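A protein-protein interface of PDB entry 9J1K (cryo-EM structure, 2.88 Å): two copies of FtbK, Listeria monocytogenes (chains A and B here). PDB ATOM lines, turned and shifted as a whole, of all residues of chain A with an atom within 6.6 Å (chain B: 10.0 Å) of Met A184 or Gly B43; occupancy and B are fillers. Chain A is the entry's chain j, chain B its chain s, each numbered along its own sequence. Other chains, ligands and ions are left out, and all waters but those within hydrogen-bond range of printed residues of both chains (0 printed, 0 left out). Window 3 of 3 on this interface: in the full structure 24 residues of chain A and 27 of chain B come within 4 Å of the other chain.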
ATOM      1  N   GLU A  37       7.252  15.733  12.856  1.00  0.00           N
ATOM      2  CA  GLU A  37       8.195  15.635  11.743  1.00  0.00           C
ATOM      3  C   GLU A  37       9.006  16.922  11.700  1.00  0.00           C
ATOM      4  O   GLU A  37       8.657  17.886  11.018  1.00  0.00           O
ATOM      5  CB  GLU A  37       7.455  15.382  10.436  1.00  0.00           C
ATOM      6  CG  GLU A  37       6.351  14.343  10.550  1.00  0.00           C
ATOM      7  CD  GLU A  37       6.802  13.086  11.270  1.00  0.00           C
ATOM      8  OE1 GLU A  37       7.842  12.513  10.882  1.00  0.00           O
ATOM      9  OE2 GLU A  37       6.117  12.671  12.230  1.00  0.00           O
ATOM     10  N   MET A  51       3.640  17.561  10.537  1.00  0.00           N
ATOM     11  CA  MET A  51       2.364  17.029  10.993  1.00  0.00           C
ATOM     12  C   MET A  51       2.640  16.019  12.098  1.00  0.00           C
ATOM     13  O   MET A  51       3.370  15.046  11.882  1.00  0.00           O
ATOM     14  CB  MET A  51       1.598  16.380   9.839  1.00  0.00           C
ATOM     15  CG  MET A  51       1.068  17.330   8.746  1.00  0.00           C
ATOM     16  SD  MET A  51       0.095  18.842   9.055  1.00  0.00           S
ATOM     17  CE  MET A  51      -0.442  18.744  10.764  1.00  0.00           C
ATOM     18  N   GLN A  53       2.522  12.947  14.358  1.00  0.00           N
ATOM     19  CA  GLN A  53       2.151  11.571  14.060  1.00  0.00           C
ATOM     20  C   GLN A  53       2.337  10.713  15.303  1.00  0.00           C
ATOM     21  O   GLN A  53       2.920  11.142  16.302  1.00  0.00           O
ATOM     22  CB  GLN A  53       2.971  11.014  12.889  1.00  0.00           C
ATOM     23  CG  GLN A  53       2.659  11.605  11.500  1.00  0.00           C
ATOM     24  CD  GLN A  53       1.184  11.572  11.111  1.00  0.00           C
ATOM     25  OE1 GLN A  53       0.805  10.871  10.180  1.00  0.00           O
ATOM     26  NE2 GLN A  53       0.364  12.378  11.771  1.00  0.00           N
ATOM     27  N   TYR A 131      -3.000   3.347  17.487  1.00  0.00           N
ATOM     28  CA  TYR A 131      -4.205   3.813  18.153  1.00  0.00           C
ATOM     29  C   TYR A 131      -5.038   2.614  18.574  1.00  0.00           C
ATOM     30  O   TYR A 131      -4.851   1.497  18.085  1.00  0.00           O
ATOM     31  CB  TYR A 131      -5.023   4.747  17.250  1.00  0.00           C
ATOM     32  CG  TYR A 131      -5.409   4.145  15.915  1.00  0.00           C
ATOM     33  CD1 TYR A 131      -6.475   3.261  15.807  1.00  0.00           C
ATOM     34  CD2 TYR A 131      -4.710   4.466  14.762  1.00  0.00           C
ATOM     35  CE1 TYR A 131      -6.829   2.713  14.592  1.00  0.00           C
ATOM     36  CE2 TYR A 131      -5.058   3.922  13.542  1.00  0.00           C
ATOM     37  CZ  TYR A 131      -6.117   3.047  13.464  1.00  0.00           C
ATOM     38  OH  TYR A 131      -6.468   2.502  12.250  1.00  0.00           O
ATOM     39  N   ASP A 178      -9.428  10.868  16.800  1.00  0.00           N
ATOM     40  CA  ASP A 178      -8.774  11.143  15.532  1.00  0.00           C
ATOM     41  C   ASP A 178      -9.825  11.424  14.472  1.00  0.00           C
ATOM     42  O   ASP A 178     -10.945  10.914  14.534  1.00  0.00           O
ATOM     43  CB  ASP A 178      -7.893   9.970  15.082  1.00  0.00           C
ATOM     44  CG  ASP A 178      -6.522   9.994  15.717  1.00  0.00           C
ATOM     45  OD1 ASP A 178      -6.434   9.803  16.948  1.00  0.00           O
ATOM     46  OD2 ASP A 178      -5.530  10.201  14.987  1.00  0.00           O
ATOM     47  N   ARG A 179      -9.450  12.242  13.494  1.00  0.00           N
ATOM     48  CA  ARG A 179     -10.325  12.500  12.361  1.00  0.00           C
ATOM     49  C   ARG A 179     -10.367  11.264  11.472  1.00  0.00           C
ATOM     50  O   ARG A 179      -9.331  10.823  10.964  1.00  0.00           O
ATOM     51  CB  ARG A 179      -9.835  13.717  11.582  1.00  0.00           C
ATOM     52  CG  ARG A 179     -10.283  13.757  10.134  1.00  0.00           C
ATOM     53  CD  ARG A 179     -10.357  15.186   9.629  1.00  0.00           C
ATOM     54  NE  ARG A 179     -10.492  15.246   8.180  1.00  0.00           N
ATOM     55  CZ  ARG A 179     -10.093  16.265   7.434  1.00  0.00           C
ATOM     56  NH1 ARG A 179      -9.529  17.334   7.970  1.00  0.00           N
ATOM     57  NH2 ARG A 179     -10.264  16.211   6.116  1.00  0.00           N
ATOM     58  N   VAL A 180     -11.558  10.698  11.295  1.00  0.00           N
ATOM     59  CA  VAL A 180     -11.693   9.462  10.532  1.00  0.00           C
ATOM     60  C   VAL A 180     -11.429   9.759   9.063  1.00  0.00           C
ATOM     61  O   VAL A 180     -12.174  10.510   8.423  1.00  0.00           O
ATOM     62  CB  VAL A 180     -13.080   8.840  10.735  1.00  0.00           C
ATOM     63  CG1 VAL A 180     -13.304   7.720   9.734  1.00  0.00           C
ATOM     64  CG2 VAL A 180     -13.224   8.326  12.156  1.00  0.00           C
ATOM     65  N   ASN A 181     -10.368   9.171   8.526  1.00  0.00           N
ATOM     66  CA  ASN A 181      -9.970   9.407   7.147  1.00  0.00           C
ATOM     67  C   ASN A 181      -9.590   8.086   6.492  1.00  0.00           C
ATOM     68  O   ASN A 181      -8.589   7.467   6.877  1.00  0.00           O
ATOM     69  CB  ASN A 181      -8.803  10.394   7.089  1.00  0.00           C
ATOM     70  CG  ASN A 181      -8.521  10.890   5.684  1.00  0.00           C
ATOM     71  OD1 ASN A 181      -9.013  10.335   4.703  1.00  0.00           O
ATOM     72  ND2 ASN A 181      -7.722  11.944   5.581  1.00  0.00           N
ATOM     73  N   PRO A 182     -10.359   7.622   5.505  1.00  0.00           N
ATOM     74  CA  PRO A 182     -10.005   6.361   4.836  1.00  0.00           C
ATOM     75  C   PRO A 182      -8.654   6.404   4.150  1.00  0.00           C
ATOM     76  O   PRO A 182      -8.028   5.353   3.966  1.00  0.00           O
ATOM     77  CB  PRO A 182     -11.147   6.169   3.829  1.00  0.00           C
ATOM     78  CG  PRO A 182     -11.712   7.532   3.623  1.00  0.00           C
ATOM     79  CD  PRO A 182     -11.570   8.235   4.935  1.00  0.00           C
ATOM     80  N   LEU A 183      -8.184   7.591   3.760  1.00  0.00           N
ATOM     81  CA  LEU A 183      -6.853   7.711   3.179  1.00  0.00           C
ATOM     82  C   LEU A 183      -5.763   7.320   4.165  1.00  0.00           C
ATOM     83  O   LEU A 183      -4.668   6.935   3.741  1.00  0.00           O
ATOM     84  CB  LEU A 183      -6.624   9.139   2.686  1.00  0.00           C
ATOM     85  CG  LEU A 183      -7.161   9.450   1.289  1.00  0.00           C
ATOM     86  CD1 LEU A 183      -6.861  10.889   0.913  1.00  0.00           C
ATOM     87  CD2 LEU A 183      -6.573   8.492   0.269  1.00  0.00           C
ATOM     88  N   MET A 184      -6.036   7.410   5.467  1.00  0.00           N
ATOM     89  CA  MET A 184      -5.100   6.993   6.503  1.00  0.00           C
ATOM     90  C   MET A 184      -5.358   5.570   6.978  1.00  0.00           C
ATOM     91  O   MET A 184      -5.090   5.251   8.144  1.00  0.00           O
ATOM     92  CB  MET A 184      -5.153   7.966   7.679  1.00  0.00           C
ATOM     93  CG  MET A 184      -5.358   9.411   7.268  1.00  0.00           C
ATOM     94  SD  MET A 184      -3.824  10.350   7.227  1.00  0.00           S
ATOM     95  CE  MET A 184      -3.773  10.977   8.903  1.00  0.00           C
ATOM     96  N   ARG A 185      -5.879   4.712   6.100  1.00  0.00           N
ATOM     97  CA  ARG A 185      -6.168   3.313   6.418  1.00  0.00           C
ATOM     98  C   ARG A 185      -7.147   3.190   7.583  1.00  0.00           C
ATOM     99  O   ARG A 185      -7.033   2.294   8.422  1.00  0.00           O
ATOM    100  CB  ARG A 185      -4.884   2.533   6.704  1.00  0.00           C
ATOM    101  CG  ARG A 185      -3.851   2.620   5.599  1.00  0.00           C
ATOM    102  CD  ARG A 185      -2.564   1.936   6.011  1.00  0.00           C
ATOM    103  NE  ARG A 185      -1.507   2.893   6.313  1.00  0.00           N
ATOM    104  CZ  ARG A 185      -1.030   3.118   7.529  1.00  0.00           C
ATOM    105  NH1 ARG A 185      -1.514   2.490   8.588  1.00  0.00           N
ATOM    106  NH2 ARG A 185      -0.040   3.990   7.686  1.00  0.00           N
ATOM    107  N   HIS A 186      -8.114   4.097   7.638  1.00  0.00           N
ATOM    108  CA  HIS A 186      -9.190   4.007   8.612  1.00  0.00           C
ATOM    109  C   HIS A 186     -10.384   3.277   8.008  1.00  0.00           C
ATOM    110  O   HIS A 186     -10.580   3.250   6.791  1.00  0.00           O
ATOM    111  CB  HIS A 186      -9.614   5.396   9.088  1.00  0.00           C
ATOM    112  CG  HIS A 186      -8.611   6.064   9.975  1.00  0.00           C
ATOM    113  ND1 HIS A 186      -8.155   7.345   9.751  1.00  0.00           N
ATOM    114  CD2 HIS A 186      -7.979   5.630  11.091  1.00  0.00           C
ATOM    115  CE1 HIS A 186      -7.284   7.671  10.688  1.00  0.00           C
ATOM    116  NE2 HIS A 186      -7.159   6.647  11.513  1.00  0.00           N
ATOM    117  N   GLU B  40       6.762   2.409   6.876  1.00  0.00           N
ATOM    118  CA  GLU B  40       6.180   3.660   7.337  1.00  0.00           C
ATOM    119  C   GLU B  40       5.734   4.500   6.149  1.00  0.00           C
ATOM    120  O   GLU B  40       6.467   4.647   5.168  1.00  0.00           O
ATOM    121  CB  GLU B  40       7.179   4.449   8.183  1.00  0.00           C
ATOM    122  CG  GLU B  40       7.062   4.202   9.675  1.00  0.00           C
ATOM    123  CD  GLU B  40       7.711   5.296  10.498  1.00  0.00           C
ATOM    124  OE1 GLU B  40       8.138   6.311   9.910  1.00  0.00           O
ATOM    125  OE2 GLU B  40       7.794   5.142  11.736  1.00  0.00           O
ATOM    126  N   ILE B  41       4.527   5.048   6.244  1.00  0.00           N
ATOM    127  CA  ILE B  41       3.977   5.938   5.230  1.00  0.00           C
ATOM    128  C   ILE B  41       3.915   7.336   5.824  1.00  0.00           C
ATOM    129  O   ILE B  41       3.298   7.544   6.876  1.00  0.00           O
ATOM    130  CB  ILE B  41       2.590   5.480   4.757  1.00  0.00           C
ATOM    131  CG1 ILE B  41       2.642   4.029   4.284  1.00  0.00           C
ATOM    132  CG2 ILE B  41       2.079   6.388   3.652  1.00  0.00           C
ATOM    133  CD1 ILE B  41       3.679   3.772   3.219  1.00  0.00           C
ATOM    134  N   ALA B  42       4.559   8.290   5.157  1.00  0.00           N
ATOM    135  CA  ALA B  42       4.517   9.669   5.617  1.00  0.00           C
ATOM    136  C   ALA B  42       3.096  10.206   5.536  1.00  0.00           C
ATOM    137  O   ALA B  42       2.379   9.967   4.560  1.00  0.00           O
ATOM    138  CB  ALA B  42       5.461  10.536   4.785  1.00  0.00           C
ATOM    139  N   GLY B  43       2.688  10.933   6.571  1.00  0.00           N
ATOM    140  CA  GLY B  43       1.350  11.472   6.645  1.00  0.00           C
ATOM    141  C   GLY B  43       0.335  10.577   7.320  1.00  0.00           C
ATOM    142  O   GLY B  43      -0.796  11.021   7.552  1.00  0.00           O
ATOM    143  N   THR B  44       0.695   9.337   7.643  1.00  0.00           N
ATOM    144  CA  THR B  44      -0.188   8.412   8.333  1.00  0.00           C
ATOM    145  C   THR B  44       0.483   7.907   9.605  1.00  0.00           C
ATOM    146  O   THR B  44       1.709   7.930   9.737  1.00  0.00           O
ATOM    147  CB  THR B  44      -0.568   7.221   7.444  1.00  0.00           C
ATOM    148  OG1 THR B  44       0.486   6.252   7.468  1.00  0.00           O
ATOM    149  CG2 THR B  44      -0.807   7.670   6.011  1.00  0.00           C
ATOM    150  N   ASP B  45      -0.339   7.445  10.542  1.00  0.00           N
ATOM    151  CA  ASP B  45       0.149   6.957  11.823  1.00  0.00           C
ATOM    152  C   ASP B  45       0.476   5.472  11.749  1.00  0.00           C
ATOM    153  O   ASP B  45      -0.067   4.734  10.923  1.00  0.00           O
ATOM    154  CB  ASP B  45      -0.882   7.197  12.926  1.00  0.00           C
ATOM    155  CG  ASP B  45      -1.279   8.650  13.048  1.00  0.00           C
ATOM    156  OD1 ASP B  45      -0.477   9.522  12.656  1.00  0.00           O
ATOM    157  OD2 ASP B  45      -2.395   8.922  13.537  1.00  0.00           O
ATOM    158  N   GLY B  46       1.377   5.042  12.628  1.00  0.00           N
ATOM    159  CA  GLY B  46       1.697   3.637  12.732  1.00  0.00           C
ATOM    160  C   GLY B  46       2.514   3.123  11.557  1.00  0.00           C
ATOM    161  O   GLY B  46       3.077   3.880  10.762  1.00  0.00           O
ATOM    162  N   VAL B  47       2.570   1.795  11.461  1.00  0.00           N
ATOM    163  CA  VAL B  47       3.322   1.108  10.422  1.00  0.00           C
ATOM    164  C   VAL B  47       2.444   0.025   9.808  1.00  0.00           C
ATOM    165  O   VAL B  47       1.453  -0.414  10.393  1.00  0.00           O
ATOM    166  CB  VAL B  47       4.630   0.486  10.956  1.00  0.00           C
ATOM    167  CG1 VAL B  47       5.488   1.539  11.636  1.00  0.00           C
ATOM    168  CG2 VAL B  47       4.320  -0.649  11.915  1.00  0.00           C
ATOM    169  N   ILE B  48       2.822  -0.396   8.607  1.00  0.00           N
ATOM    170  CA  ILE B  48       2.194  -1.524   7.926  1.00  0.00           C
ATOM    171  C   ILE B  48       3.128  -2.721   8.057  1.00  0.00           C
ATOM    172  O   ILE B  48       4.289  -2.632   7.632  1.00  0.00           O
ATOM    173  CB  ILE B  48       1.907  -1.213   6.451  1.00  0.00           C
ATOM    174  CG1 ILE B  48       0.797  -0.173   6.335  1.00  0.00           C
ATOM    175  CG2 ILE B  48       1.521  -2.480   5.709  1.00  0.00           C
ATOM    176  CD1 ILE B  48       1.291   1.171   5.891  1.00  0.00           C
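The side-chain amide oxygen (OE1) of Gln A53 sits close to the backbone carbonyl oxygen (O) of Gly B43 (3.1 Å). N of Thr B44 sits at hydrogen-bond distance from OE1 of Gln A53 (3.0 Å). The side-chain amide oxygen (OE1) of Gln A53 lies close to the side-chain carboxylate (OD1) of Asp B45, at 3.1 Å. The backbone carbonyl oxygen (O) of Asp B45 is in hydrogen-bond range of the guanidinium group (NH2) of Arg A185 (3.3 Å). The side-chain sulfur (SD) of Met A184 lies close to the backbone carbonyl oxygen (O) of Gly B43, 3.1 Å away. NH2 of Arg A185 sits close to OG1 of Thr B44, 2.3 Å away.
The side-chain hydroxyl (OG1) of Thr B44 sits at hydrogen-bond distance from the backbone carbonyl oxygen (O) of Ile B41.
Asp A178 touches Asp B45. Arg A185 touches Ile B48 (NE to CD1, 3.3 Å).
Printed residues of chain B within 4 Å of Asp A178: Asp B45 (3.7 Å). Met A184 touches just one residue of chain B: Gly B43. Arg A185 touches just these residues of chain B: Thr B44 (2.3 Å), Asp B45 (3.3 Å) and Ile B48 (3.3 Å). No residue of chain B comes within 4 Å of His A186. Ala B42 touches none of the printed residues of chain A. Of chain A, only Gln A53 and Met A184 come within 4 Å of Gly B43. Printed residues of chain A within 4 Å of Thr B44: Gln A53 and Arg A185. Printed residues of chain A within 4 Å of Asp B45: Gln A53 (3.1 Å), Asp A178 (3.7 Å) and Arg A185 (3.3 Å). Of the printed residues of chain A, Ile B48 touches Arg A185 (3.3 Å). The nearest residue of chain B that does not touch Met A184 is Thr B44 (4.2 Å). The nearest residue of chain A that does not touch Gly B43 is Met A51 (5.9 Å). The nearest printed residue of chain A that does not touch Thr B44 is Met A184 (4.2 Å).
Of the 13 printed residues of chain A, 4 touch a printed residue of chain B. Hydrophobic or aromatic side chains of chain A within 4 Å of the printed part of chain B: Met A184. Printed residues of chain B that touch a printed residue of chain A: Gly B43, Thr B44, Asp B45 and Ile B48. Hydrophobic or aromatic side chains of chain B that line the printed part of chain A: Ile B48. Among the printed residues, 8 pairs touch across the chains. Among the printed residues, no Asp or Glu carboxylate lies within 4 Å of a Lys or Arg side-chain nitrogen of the other chain.
No position is printed for both chains.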
